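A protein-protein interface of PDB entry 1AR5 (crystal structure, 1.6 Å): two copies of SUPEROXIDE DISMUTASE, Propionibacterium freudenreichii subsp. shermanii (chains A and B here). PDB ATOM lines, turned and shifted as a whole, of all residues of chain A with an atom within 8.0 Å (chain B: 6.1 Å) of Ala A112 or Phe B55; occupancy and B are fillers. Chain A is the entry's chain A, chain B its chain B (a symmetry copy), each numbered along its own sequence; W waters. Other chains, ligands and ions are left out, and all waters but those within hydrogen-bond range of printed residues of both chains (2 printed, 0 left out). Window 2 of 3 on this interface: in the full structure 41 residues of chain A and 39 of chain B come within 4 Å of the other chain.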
ATOM      1  N   PHE A 104      -1.413  11.091   9.122  1.00  0.00           N
ATOM      2  CA  PHE A 104      -1.718  10.210  10.249  1.00  0.00           C
ATOM      3  C   PHE A 104      -2.459   8.941   9.840  1.00  0.00           C
ATOM      4  O   PHE A 104      -2.613   8.019  10.642  1.00  0.00           O
ATOM      5  CB  PHE A 104      -2.536  10.955  11.309  1.00  0.00           C
ATOM      6  CG  PHE A 104      -1.818  12.124  11.924  1.00  0.00           C
ATOM      7  CD1 PHE A 104      -0.999  11.947  13.035  1.00  0.00           C
ATOM      8  CD2 PHE A 104      -1.964  13.401  11.394  1.00  0.00           C
ATOM      9  CE1 PHE A 104      -0.337  13.026  13.607  1.00  0.00           C
ATOM     10  CE2 PHE A 104      -1.306  14.487  11.960  1.00  0.00           C
ATOM     11  CZ  PHE A 104      -0.493  14.300  13.069  1.00  0.00           C
ATOM     12  N   SER A 106      -5.599   8.477   9.316  1.00  0.00           N
ATOM     13  CA  SER A 106      -7.013   8.732   9.552  1.00  0.00           C
ATOM     14  C   SER A 106      -7.183   9.658  10.745  1.00  0.00           C
ATOM     15  O   SER A 106      -6.245   9.866  11.520  1.00  0.00           O
ATOM     16  CB  SER A 106      -7.758   7.421   9.828  1.00  0.00           C
ATOM     17  OG  SER A 106      -7.294   6.804  11.019  1.00  0.00           O
ATOM     18  N   PHE A 107      -8.390  10.197  10.894  1.00  0.00           N
ATOM     19  CA  PHE A 107      -8.707  11.087  12.003  1.00  0.00           C
ATOM     20  C   PHE A 107      -8.558  10.331  13.317  1.00  0.00           C
ATOM     21  O   PHE A 107      -8.019  10.861  14.283  1.00  0.00           O
ATOM     22  CB  PHE A 107     -10.137  11.620  11.872  1.00  0.00           C
ATOM     23  CG  PHE A 107     -10.586  12.451  13.041  1.00  0.00           C
ATOM     24  CD1 PHE A 107      -9.912  13.618  13.385  1.00  0.00           C
ATOM     25  CD2 PHE A 107     -11.681  12.063  13.804  1.00  0.00           C
ATOM     26  CE1 PHE A 107     -10.325  14.388  14.471  1.00  0.00           C
ATOM     27  CE2 PHE A 107     -12.102  12.826  14.890  1.00  0.00           C
ATOM     28  CZ  PHE A 107     -11.422  13.991  15.225  1.00  0.00           C
ATOM     29  N   ASP A 108      -9.024   9.085  13.335  1.00  0.00           N
ATOM     30  CA  ASP A 108      -8.947   8.253  14.531  1.00  0.00           C
ATOM     31  C   ASP A 108      -7.513   7.994  14.975  1.00  0.00           C
ATOM     32  O   ASP A 108      -7.236   7.947  16.173  1.00  0.00           O
ATOM     33  CB  ASP A 108      -9.692   6.931  14.321  1.00  0.00           C
ATOM     34  CG  ASP A 108     -11.197   7.058  14.538  1.00  0.00           C
ATOM     35  OD1 ASP A 108     -11.732   8.189  14.507  1.00  0.00           O
ATOM     36  OD2 ASP A 108     -11.849   6.013  14.749  1.00  0.00           O
ATOM     37  N   ASN A 109      -6.605   7.829  14.014  1.00  0.00           N
ATOM     38  CA  ASN A 109      -5.194   7.594  14.324  1.00  0.00           C
ATOM     39  C   ASN A 109      -4.565   8.838  14.939  1.00  0.00           C
ATOM     40  O   ASN A 109      -3.771   8.743  15.875  1.00  0.00           O
ATOM     41  CB  ASN A 109      -4.420   7.193  13.069  1.00  0.00           C
ATOM     42  CG  ASN A 109      -4.643   5.745  12.676  1.00  0.00           C
ATOM     43  OD1 ASN A 109      -5.310   4.991  13.384  1.00  0.00           O
ATOM     44  ND2 ASN A 109      -4.077   5.348  11.544  1.00  0.00           N
ATOM     45  N   MET A 110      -4.912  10.003  14.397  1.00  0.00           N
ATOM     46  CA  MET A 110      -4.397  11.275  14.894  1.00  0.00           C
ATOM     47  C   MET A 110      -4.896  11.505  16.315  1.00  0.00           C
ATOM     48  O   MET A 110      -4.143  11.931  17.186  1.00  0.00           O
ATOM     49  CB  MET A 110      -4.857  12.419  13.983  1.00  0.00           C
ATOM     50  CG  MET A 110      -4.353  13.805  14.370  1.00  0.00           C
ATOM     51  SD  MET A 110      -5.225  14.551  15.756  1.00  0.00           S
ATOM     52  CE  MET A 110      -6.549  15.368  14.907  1.00  0.00           C
ATOM     53  N   LYS A 111      -6.171  11.200  16.540  1.00  0.00           N
ATOM     54  CA  LYS A 111      -6.798  11.365  17.845  1.00  0.00           C
ATOM     55  C   LYS A 111      -6.135  10.472  18.888  1.00  0.00           C
ATOM     56  O   LYS A 111      -5.886  10.907  20.011  1.00  0.00           O
ATOM     57  CB  LYS A 111      -8.296  11.061  17.745  1.00  0.00           C
ATOM     58  CG  LYS A 111      -9.071  11.260  19.031  1.00  0.00           C
ATOM     59  CD  LYS A 111     -10.574  11.227  18.774  1.00  0.00           C
ATOM     60  CE  LYS A 111     -11.356  11.307  20.071  1.00  0.00           C
ATOM     61  NZ  LYS A 111     -12.827  11.336  19.855  1.00  0.00           N
ATOM     62  N   ALA A 112      -5.823   9.238  18.503  1.00  0.00           N
ATOM     63  CA  ALA A 112      -5.179   8.290  19.410  1.00  0.00           C
ATOM     64  C   ALA A 112      -3.764   8.743  19.765  1.00  0.00           C
ATOM     65  O   ALA A 112      -3.369   8.699  20.930  1.00  0.00           O
ATOM     66  CB  ALA A 112      -5.149   6.898  18.789  1.00  0.00           C
ATOM     67  N   GLN A 113      -3.013   9.193  18.760  1.00  0.00           N
ATOM     68  CA  GLN A 113      -1.641   9.657  18.966  1.00  0.00           C
ATOM     69  C   GLN A 113      -1.614  10.911  19.829  1.00  0.00           C
ATOM     70  O   GLN A 113      -0.806  11.018  20.752  1.00  0.00           O
ATOM     71  CB  GLN A 113      -0.947   9.928  17.624  1.00  0.00           C
ATOM     72  CG  GLN A 113       0.520  10.328  17.754  1.00  0.00           C
ATOM     73  CD  GLN A 113       1.251  10.368  16.424  1.00  0.00           C
ATOM     74  OE1 GLN A 113       2.036  11.281  16.161  1.00  0.00           O
ATOM     75  NE2 GLN A 113       1.019   9.364  15.589  1.00  0.00           N
ATOM     76  N   PHE A 114      -2.527  11.836  19.543  1.00  0.00           N
ATOM     77  CA  PHE A 114      -2.632  13.095  20.274  1.00  0.00           C
ATOM     78  C   PHE A 114      -3.017  12.838  21.734  1.00  0.00           C
ATOM     79  O   PHE A 114      -2.453  13.443  22.647  1.00  0.00           O
ATOM     80  CB  PHE A 114      -3.665  14.003  19.594  1.00  0.00           C
ATOM     81  CG  PHE A 114      -3.711  15.405  20.141  1.00  0.00           C
ATOM     82  CD1 PHE A 114      -4.412  15.693  21.308  1.00  0.00           C
ATOM     83  CD2 PHE A 114      -3.068  16.442  19.477  1.00  0.00           C
ATOM     84  CE1 PHE A 114      -4.473  16.991  21.803  1.00  0.00           C
ATOM     85  CE2 PHE A 114      -3.123  17.743  19.964  1.00  0.00           C
ATOM     86  CZ  PHE A 114      -3.827  18.018  21.131  1.00  0.00           C
ATOM     87  N   THR A 115      -3.962  11.925  21.944  1.00  0.00           N
ATOM     88  CA  THR A 115      -4.419  11.580  23.289  1.00  0.00           C
ATOM     89  C   THR A 115      -3.293  10.951  24.106  1.00  0.00           C
ATOM     90  O   THR A 115      -3.113  11.281  25.279  1.00  0.00           O
ATOM     91  CB  THR A 115      -5.618  10.617  23.238  1.00  0.00           C
ATOM     92  OG1 THR A 115      -6.725  11.273  22.604  1.00  0.00           O
ATOM     93  CG2 THR A 115      -6.024  10.182  24.643  1.00  0.00           C
ATOM     94  N   ALA A 116      -2.531  10.060  23.477  1.00  0.00           N
ATOM     95  CA  ALA A 116      -1.415   9.392  24.139  1.00  0.00           C
ATOM     96  C   ALA A 116      -0.355  10.412  24.540  1.00  0.00           C
ATOM     97  O   ALA A 116       0.200  10.346  25.638  1.00  0.00           O
ATOM     98  CB  ALA A 116      -0.818   8.336  23.225  1.00  0.00           C
ATOM     99  N   ALA A 117      -0.108  11.380  23.663  1.00  0.00           N
ATOM    100  CA  ALA A 117       0.875  12.426  23.928  1.00  0.00           C
ATOM    101  C   ALA A 117       0.419  13.302  25.090  1.00  0.00           C
ATOM    102  O   ALA A 117       1.230  13.773  25.885  1.00  0.00           O
ATOM    103  CB  ALA A 117       1.080  13.277  22.680  1.00  0.00           C
ATOM    104  N   ALA A 118      -0.890  13.495  25.195  1.00  0.00           N
ATOM    105  CA  ALA A 118      -1.463  14.326  26.241  1.00  0.00           C
ATOM    106  C   ALA A 118      -1.446  13.696  27.627  1.00  0.00           C
ATOM    107  O   ALA A 118      -1.081  14.351  28.602  1.00  0.00           O
ATOM    108  CB  ALA A 118      -2.885  14.721  25.866  1.00  0.00           C
ATOM    109  N   THR A 119      -1.831  12.427  27.713  1.00  0.00           N
ATOM    110  CA  THR A 119      -1.892  11.742  28.999  1.00  0.00           C
ATOM    111  C   THR A 119      -0.563  11.211  29.529  1.00  0.00           C
ATOM    112  O   THR A 119      -0.432  10.964  30.727  1.00  0.00           O
ATOM    113  CB  THR A 119      -2.918  10.595  28.975  1.00  0.00           C
ATOM    114  OG1 THR A 119      -2.526   9.617  28.007  1.00  0.00           O
ATOM    115  CG2 THR A 119      -4.296  11.124  28.613  1.00  0.00           C
ATOM    116  N   GLY A 120       0.425  11.067  28.652  1.00  0.00           N
ATOM    117  CA  GLY A 120       1.717  10.551  29.077  1.00  0.00           C
ATOM    118  C   GLY A 120       2.733  11.554  29.595  1.00  0.00           C
ATOM    119  O   GLY A 120       3.801  11.156  30.060  1.00  0.00           O
ATOM    120  N   THR A 140       2.654  15.834  15.728  1.00  0.00           N
ATOM    121  CA  THR A 140       2.169  16.028  17.087  1.00  0.00           C
ATOM    122  C   THR A 140       3.435  16.228  17.909  1.00  0.00           C
ATOM    123  O   THR A 140       4.448  15.566  17.667  1.00  0.00           O
ATOM    124  CB  THR A 140       1.413  14.802  17.654  1.00  0.00           C
ATOM    125  OG1 THR A 140       2.214  13.625  17.505  1.00  0.00           O
ATOM    126  CG2 THR A 140       0.072  14.618  16.959  1.00  0.00           C
ATOM    127  N   TRP A 183     -12.400  16.761  23.649  1.00  0.00           N
ATOM    128  CA  TRP A 183     -12.631  16.525  22.225  1.00  0.00           C
ATOM    129  C   TRP A 183     -13.983  17.058  21.754  1.00  0.00           C
ATOM    130  O   TRP A 183     -14.129  17.453  20.598  1.00  0.00           O
ATOM    131  CB  TRP A 183     -12.506  15.036  21.888  1.00  0.00           C
ATOM    132  CG  TRP A 183     -11.089  14.545  21.843  1.00  0.00           C
ATOM    133  CD1 TRP A 183     -10.490  13.679  22.713  1.00  0.00           C
ATOM    134  CD2 TRP A 183     -10.087  14.902  20.880  1.00  0.00           C
ATOM    135  NE1 TRP A 183      -9.180  13.474  22.353  1.00  0.00           N
ATOM    136  CE2 TRP A 183      -8.905  14.212  21.233  1.00  0.00           C
ATOM    137  CE3 TRP A 183     -10.074  15.737  19.754  1.00  0.00           C
ATOM    138  CZ2 TRP A 183      -7.718  14.333  20.500  1.00  0.00           C
ATOM    139  CZ3 TRP A 183      -8.890  15.857  19.024  1.00  0.00           C
ATOM    140  CH2 TRP A 183      -7.730  15.157  19.404  1.00  0.00           C
ATOM    141  N   LEU B  46       6.868   6.576  14.874  1.00  0.00           N
ATOM    142  CA  LEU B  46       5.535   7.078  15.196  1.00  0.00           C
ATOM    143  C   LEU B  46       4.503   6.470  14.251  1.00  0.00           C
ATOM    144  O   LEU B  46       3.385   6.162  14.658  1.00  0.00           O
ATOM    145  CB  LEU B  46       5.493   8.605  15.109  1.00  0.00           C
ATOM    146  CG  LEU B  46       6.092   9.368  16.292  1.00  0.00           C
ATOM    147  CD1 LEU B  46       6.277  10.836  15.937  1.00  0.00           C
ATOM    148  CD2 LEU B  46       5.196   9.212  17.516  1.00  0.00           C
ATOM    149  N   ALA B  49       3.856   3.047  15.376  1.00  0.00           N
ATOM    150  CA  ALA B  49       3.074   3.089  16.606  1.00  0.00           C
ATOM    151  C   ALA B  49       1.584   3.161  16.281  1.00  0.00           C
ATOM    152  O   ALA B  49       0.776   2.478  16.904  1.00  0.00           O
ATOM    153  CB  ALA B  49       3.485   4.283  17.450  1.00  0.00           C
ATOM    154  N   ARG B  50       1.232   3.979  15.291  1.00  0.00           N
ATOM    155  CA  ARG B  50      -0.157   4.135  14.871  1.00  0.00           C
ATOM    156  C   ARG B  50      -0.710   2.866  14.233  1.00  0.00           C
ATOM    157  O   ARG B  50      -1.849   2.483  14.493  1.00  0.00           O
ATOM    158  CB  ARG B  50      -0.302   5.295  13.884  1.00  0.00           C
ATOM    159  CG  ARG B  50      -0.088   6.670  14.484  1.00  0.00           C
ATOM    160  CD  ARG B  50      -0.438   7.756  13.480  1.00  0.00           C
ATOM    161  NE  ARG B  50       0.345   7.643  12.251  1.00  0.00           N
ATOM    162  CZ  ARG B  50       1.459   8.324  12.005  1.00  0.00           C
ATOM    163  NH1 ARG B  50       1.939   9.179  12.901  1.00  0.00           N
ATOM    164  NH2 ARG B  50       2.092   8.157  10.853  1.00  0.00           N
ATOM    165  N   ALA B  53      -1.143   0.458  16.885  1.00  0.00           N
ATOM    166  CA  ALA B  53      -2.044   1.009  17.900  1.00  0.00           C
ATOM    167  C   ALA B  53      -1.450   0.929  19.307  1.00  0.00           C
ATOM    168  O   ALA B  53      -2.178   0.845  20.299  1.00  0.00           O
ATOM    169  CB  ALA B  53      -3.407   0.311  17.848  1.00  0.00           C
ATOM    170  N   ASP B  54      -0.123   0.975  19.383  1.00  0.00           N
ATOM    171  CA  ASP B  54       0.588   0.904  20.655  1.00  0.00           C
ATOM    172  C   ASP B  54       1.453   2.150  20.821  1.00  0.00           C
ATOM    173  O   ASP B  54       2.491   2.284  20.175  1.00  0.00           O
ATOM    174  CB  ASP B  54       1.462  -0.357  20.689  1.00  0.00           C
ATOM    175  CG  ASP B  54       2.120  -0.590  22.044  1.00  0.00           C
ATOM    176  OD1 ASP B  54       1.913   0.208  22.980  1.00  0.00           O
ATOM    177  OD2 ASP B  54       2.853  -1.594  22.171  1.00  0.00           O
ATOM    178  N   PHE B  55       1.022   3.052  21.696  1.00  0.00           N
ATOM    179  CA  PHE B  55       1.750   4.293  21.945  1.00  0.00           C
ATOM    180  C   PHE B  55       2.506   4.275  23.271  1.00  0.00           C
ATOM    181  O   PHE B  55       2.657   5.307  23.923  1.00  0.00           O
ATOM    182  CB  PHE B  55       0.791   5.487  21.902  1.00  0.00           C
ATOM    183  CG  PHE B  55       0.089   5.648  20.588  1.00  0.00           C
ATOM    184  CD1 PHE B  55       0.692   6.340  19.543  1.00  0.00           C
ATOM    185  CD2 PHE B  55      -1.170   5.093  20.387  1.00  0.00           C
ATOM    186  CE1 PHE B  55       0.053   6.474  18.313  1.00  0.00           C
ATOM    187  CE2 PHE B  55      -1.819   5.220  19.163  1.00  0.00           C
ATOM    188  CZ  PHE B  55      -1.206   5.912  18.123  1.00  0.00           C
ATOM    189  N   GLY B  56       3.002   3.099  23.648  1.00  0.00           N
ATOM    190  CA  GLY B  56       3.735   2.961  24.894  1.00  0.00           C
ATOM    191  C   GLY B  56       5.000   3.797  24.980  1.00  0.00           C
ATOM    192  O   GLY B  56       5.366   4.259  26.059  1.00  0.00           O
ATOM    193  N   ALA B  57       5.659   4.010  23.846  1.00  0.00           N
ATOM    194  CA  ALA B  57       6.891   4.788  23.817  1.00  0.00           C
ATOM    195  C   ALA B  57       6.691   6.218  23.320  1.00  0.00           C
ATOM    196  O   ALA B  57       7.649   6.869  22.909  1.00  0.00           O
ATOM    197  CB  ALA B  57       7.930   4.081  22.961  1.00  0.00           C
ATOM    198  N   ILE B  58       5.458   6.716  23.397  1.00  0.00           N
ATOM    199  CA  ILE B  58       5.136   8.067  22.933  1.00  0.00           C
ATOM    200  C   ILE B  58       6.018   9.179  23.523  1.00  0.00           C
ATOM    201  O   ILE B  58       6.424  10.091  22.802  1.00  0.00           O
ATOM    202  CB  ILE B  58       3.625   8.397  23.146  1.00  0.00           C
ATOM    203  CG1 ILE B  58       3.249   9.704  22.436  1.00  0.00           C
ATOM    204  CG2 ILE B  58       3.290   8.478  24.628  1.00  0.00           C
ATOM    205  CD1 ILE B  58       3.296   9.630  20.922  1.00  0.00           C
ATOM    206  N   ASN B  59       6.337   9.098  24.815  1.00  0.00           N
ATOM    207  CA  ASN B  59       7.176  10.115  25.450  1.00  0.00           C
ATOM    208  C   ASN B  59       8.580  10.138  24.844  1.00  0.00           C
ATOM    209  O   ASN B  59       9.152  11.205  24.612  1.00  0.00           O
ATOM    210  CB  ASN B  59       7.258   9.888  26.965  1.00  0.00           C
ATOM    211  CG  ASN B  59       5.938  10.164  27.675  1.00  0.00           C
ATOM    212  OD1 ASN B  59       5.010  10.732  27.098  1.00  0.00           O
ATOM    213  ND2 ASN B  59       5.854   9.764  28.938  1.00  0.00           N
HETATM  214  O   HOH W   1       3.718  11.506  13.146  1.00  0.00           O
HETATM  215  O   HOH W   2      -3.765   4.322  16.228  1.00  0.00           O
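The guanidinium group (NE) of Arg B50 sits at hydrogen-bond distance from the backbone carbonyl oxygen (O) of Phe A104, at 3.4 Å.
ND2 of Asn B59 is in hydrogen-bond range of O of Gly A120 (2.7 Å).
NE2 of Gln A113 sits close to NH1 of Arg B50 (2.8 Å).
The side-chain amide oxygen (OE1) of Gln A113 sits at hydrogen-bond distance from the side-chain hydroxyl (OG1) of Thr A140.
The backbone carbonyl oxygen (O) of Phe A104 lies close to the side-chain amide nitrogen (ND2) of Asn A109.
Among the printed residues, merely in contact across the chains: Ala A116 with Phe B55 (3.5 Å), Gln A113 with Phe B55 (3.7 Å), Ala A112 with Phe B55 (3.7 Å), Ala A116 with Ile B58 (3.7 Å) and Ala A117 with Ile B58 (3.9 Å).
Of chain B, only Phe B55 comes within 4 Å of Ala A112.
Of chain A, only Ala A112 (3.7 Å), Gln A113 (3.7 Å) and Ala A116 (3.5 Å) come within 4 Å of Phe B55.
No residue of chain A comes within 4 Å of Gly B56.
Of the printed residues of chain A, Ile B58 touches Ala A116 and Ala A117.
Printed residues of chain B within 4 Å of Ala A116: Phe B55 and Ile B58.
Of the printed residues of chain B, Ala A117 touches Ile B58.
Ala B49 touches none of the printed residues of chain A.
Lys A111 touches none of the printed residues of chain B.
The nearest printed residue of chain B that does not touch Ala A112 is Arg B50 (6.6 Å).
The nearest printed residue of chain A that does not touch Ile B58 is Gln A113 (4.3 Å).
Of the 10 printed residues of chain B, 4 touch a printed residue of chain A.
Printed residues of chain B that touch a printed residue of chain A: Arg B50, Phe B55, Ile B58 and Asn B59.
Printed residues of chain A that touch a printed residue of chain B: Phe A104, Ala A112, Gln A113, Ala A116, Ala A117 and Gly A120.
Among the printed residues, 8 pairs touch across the chains.
Among the printed residues, no Asp or Glu carboxylate lies within 4 Å of a Lys or Arg side-chain nitrogen of the other chain.
No position is printed for both chains.
Water W1 lies within hydrogen-bond range of the guanidinium group (NH1) of Arg B50 and the side-chain amide oxygen (OE1) of Gln A113.
Water W2 bridges O of Arg B50 (3.2 Å) and OD1 of Asn A109 (3.3 Å).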
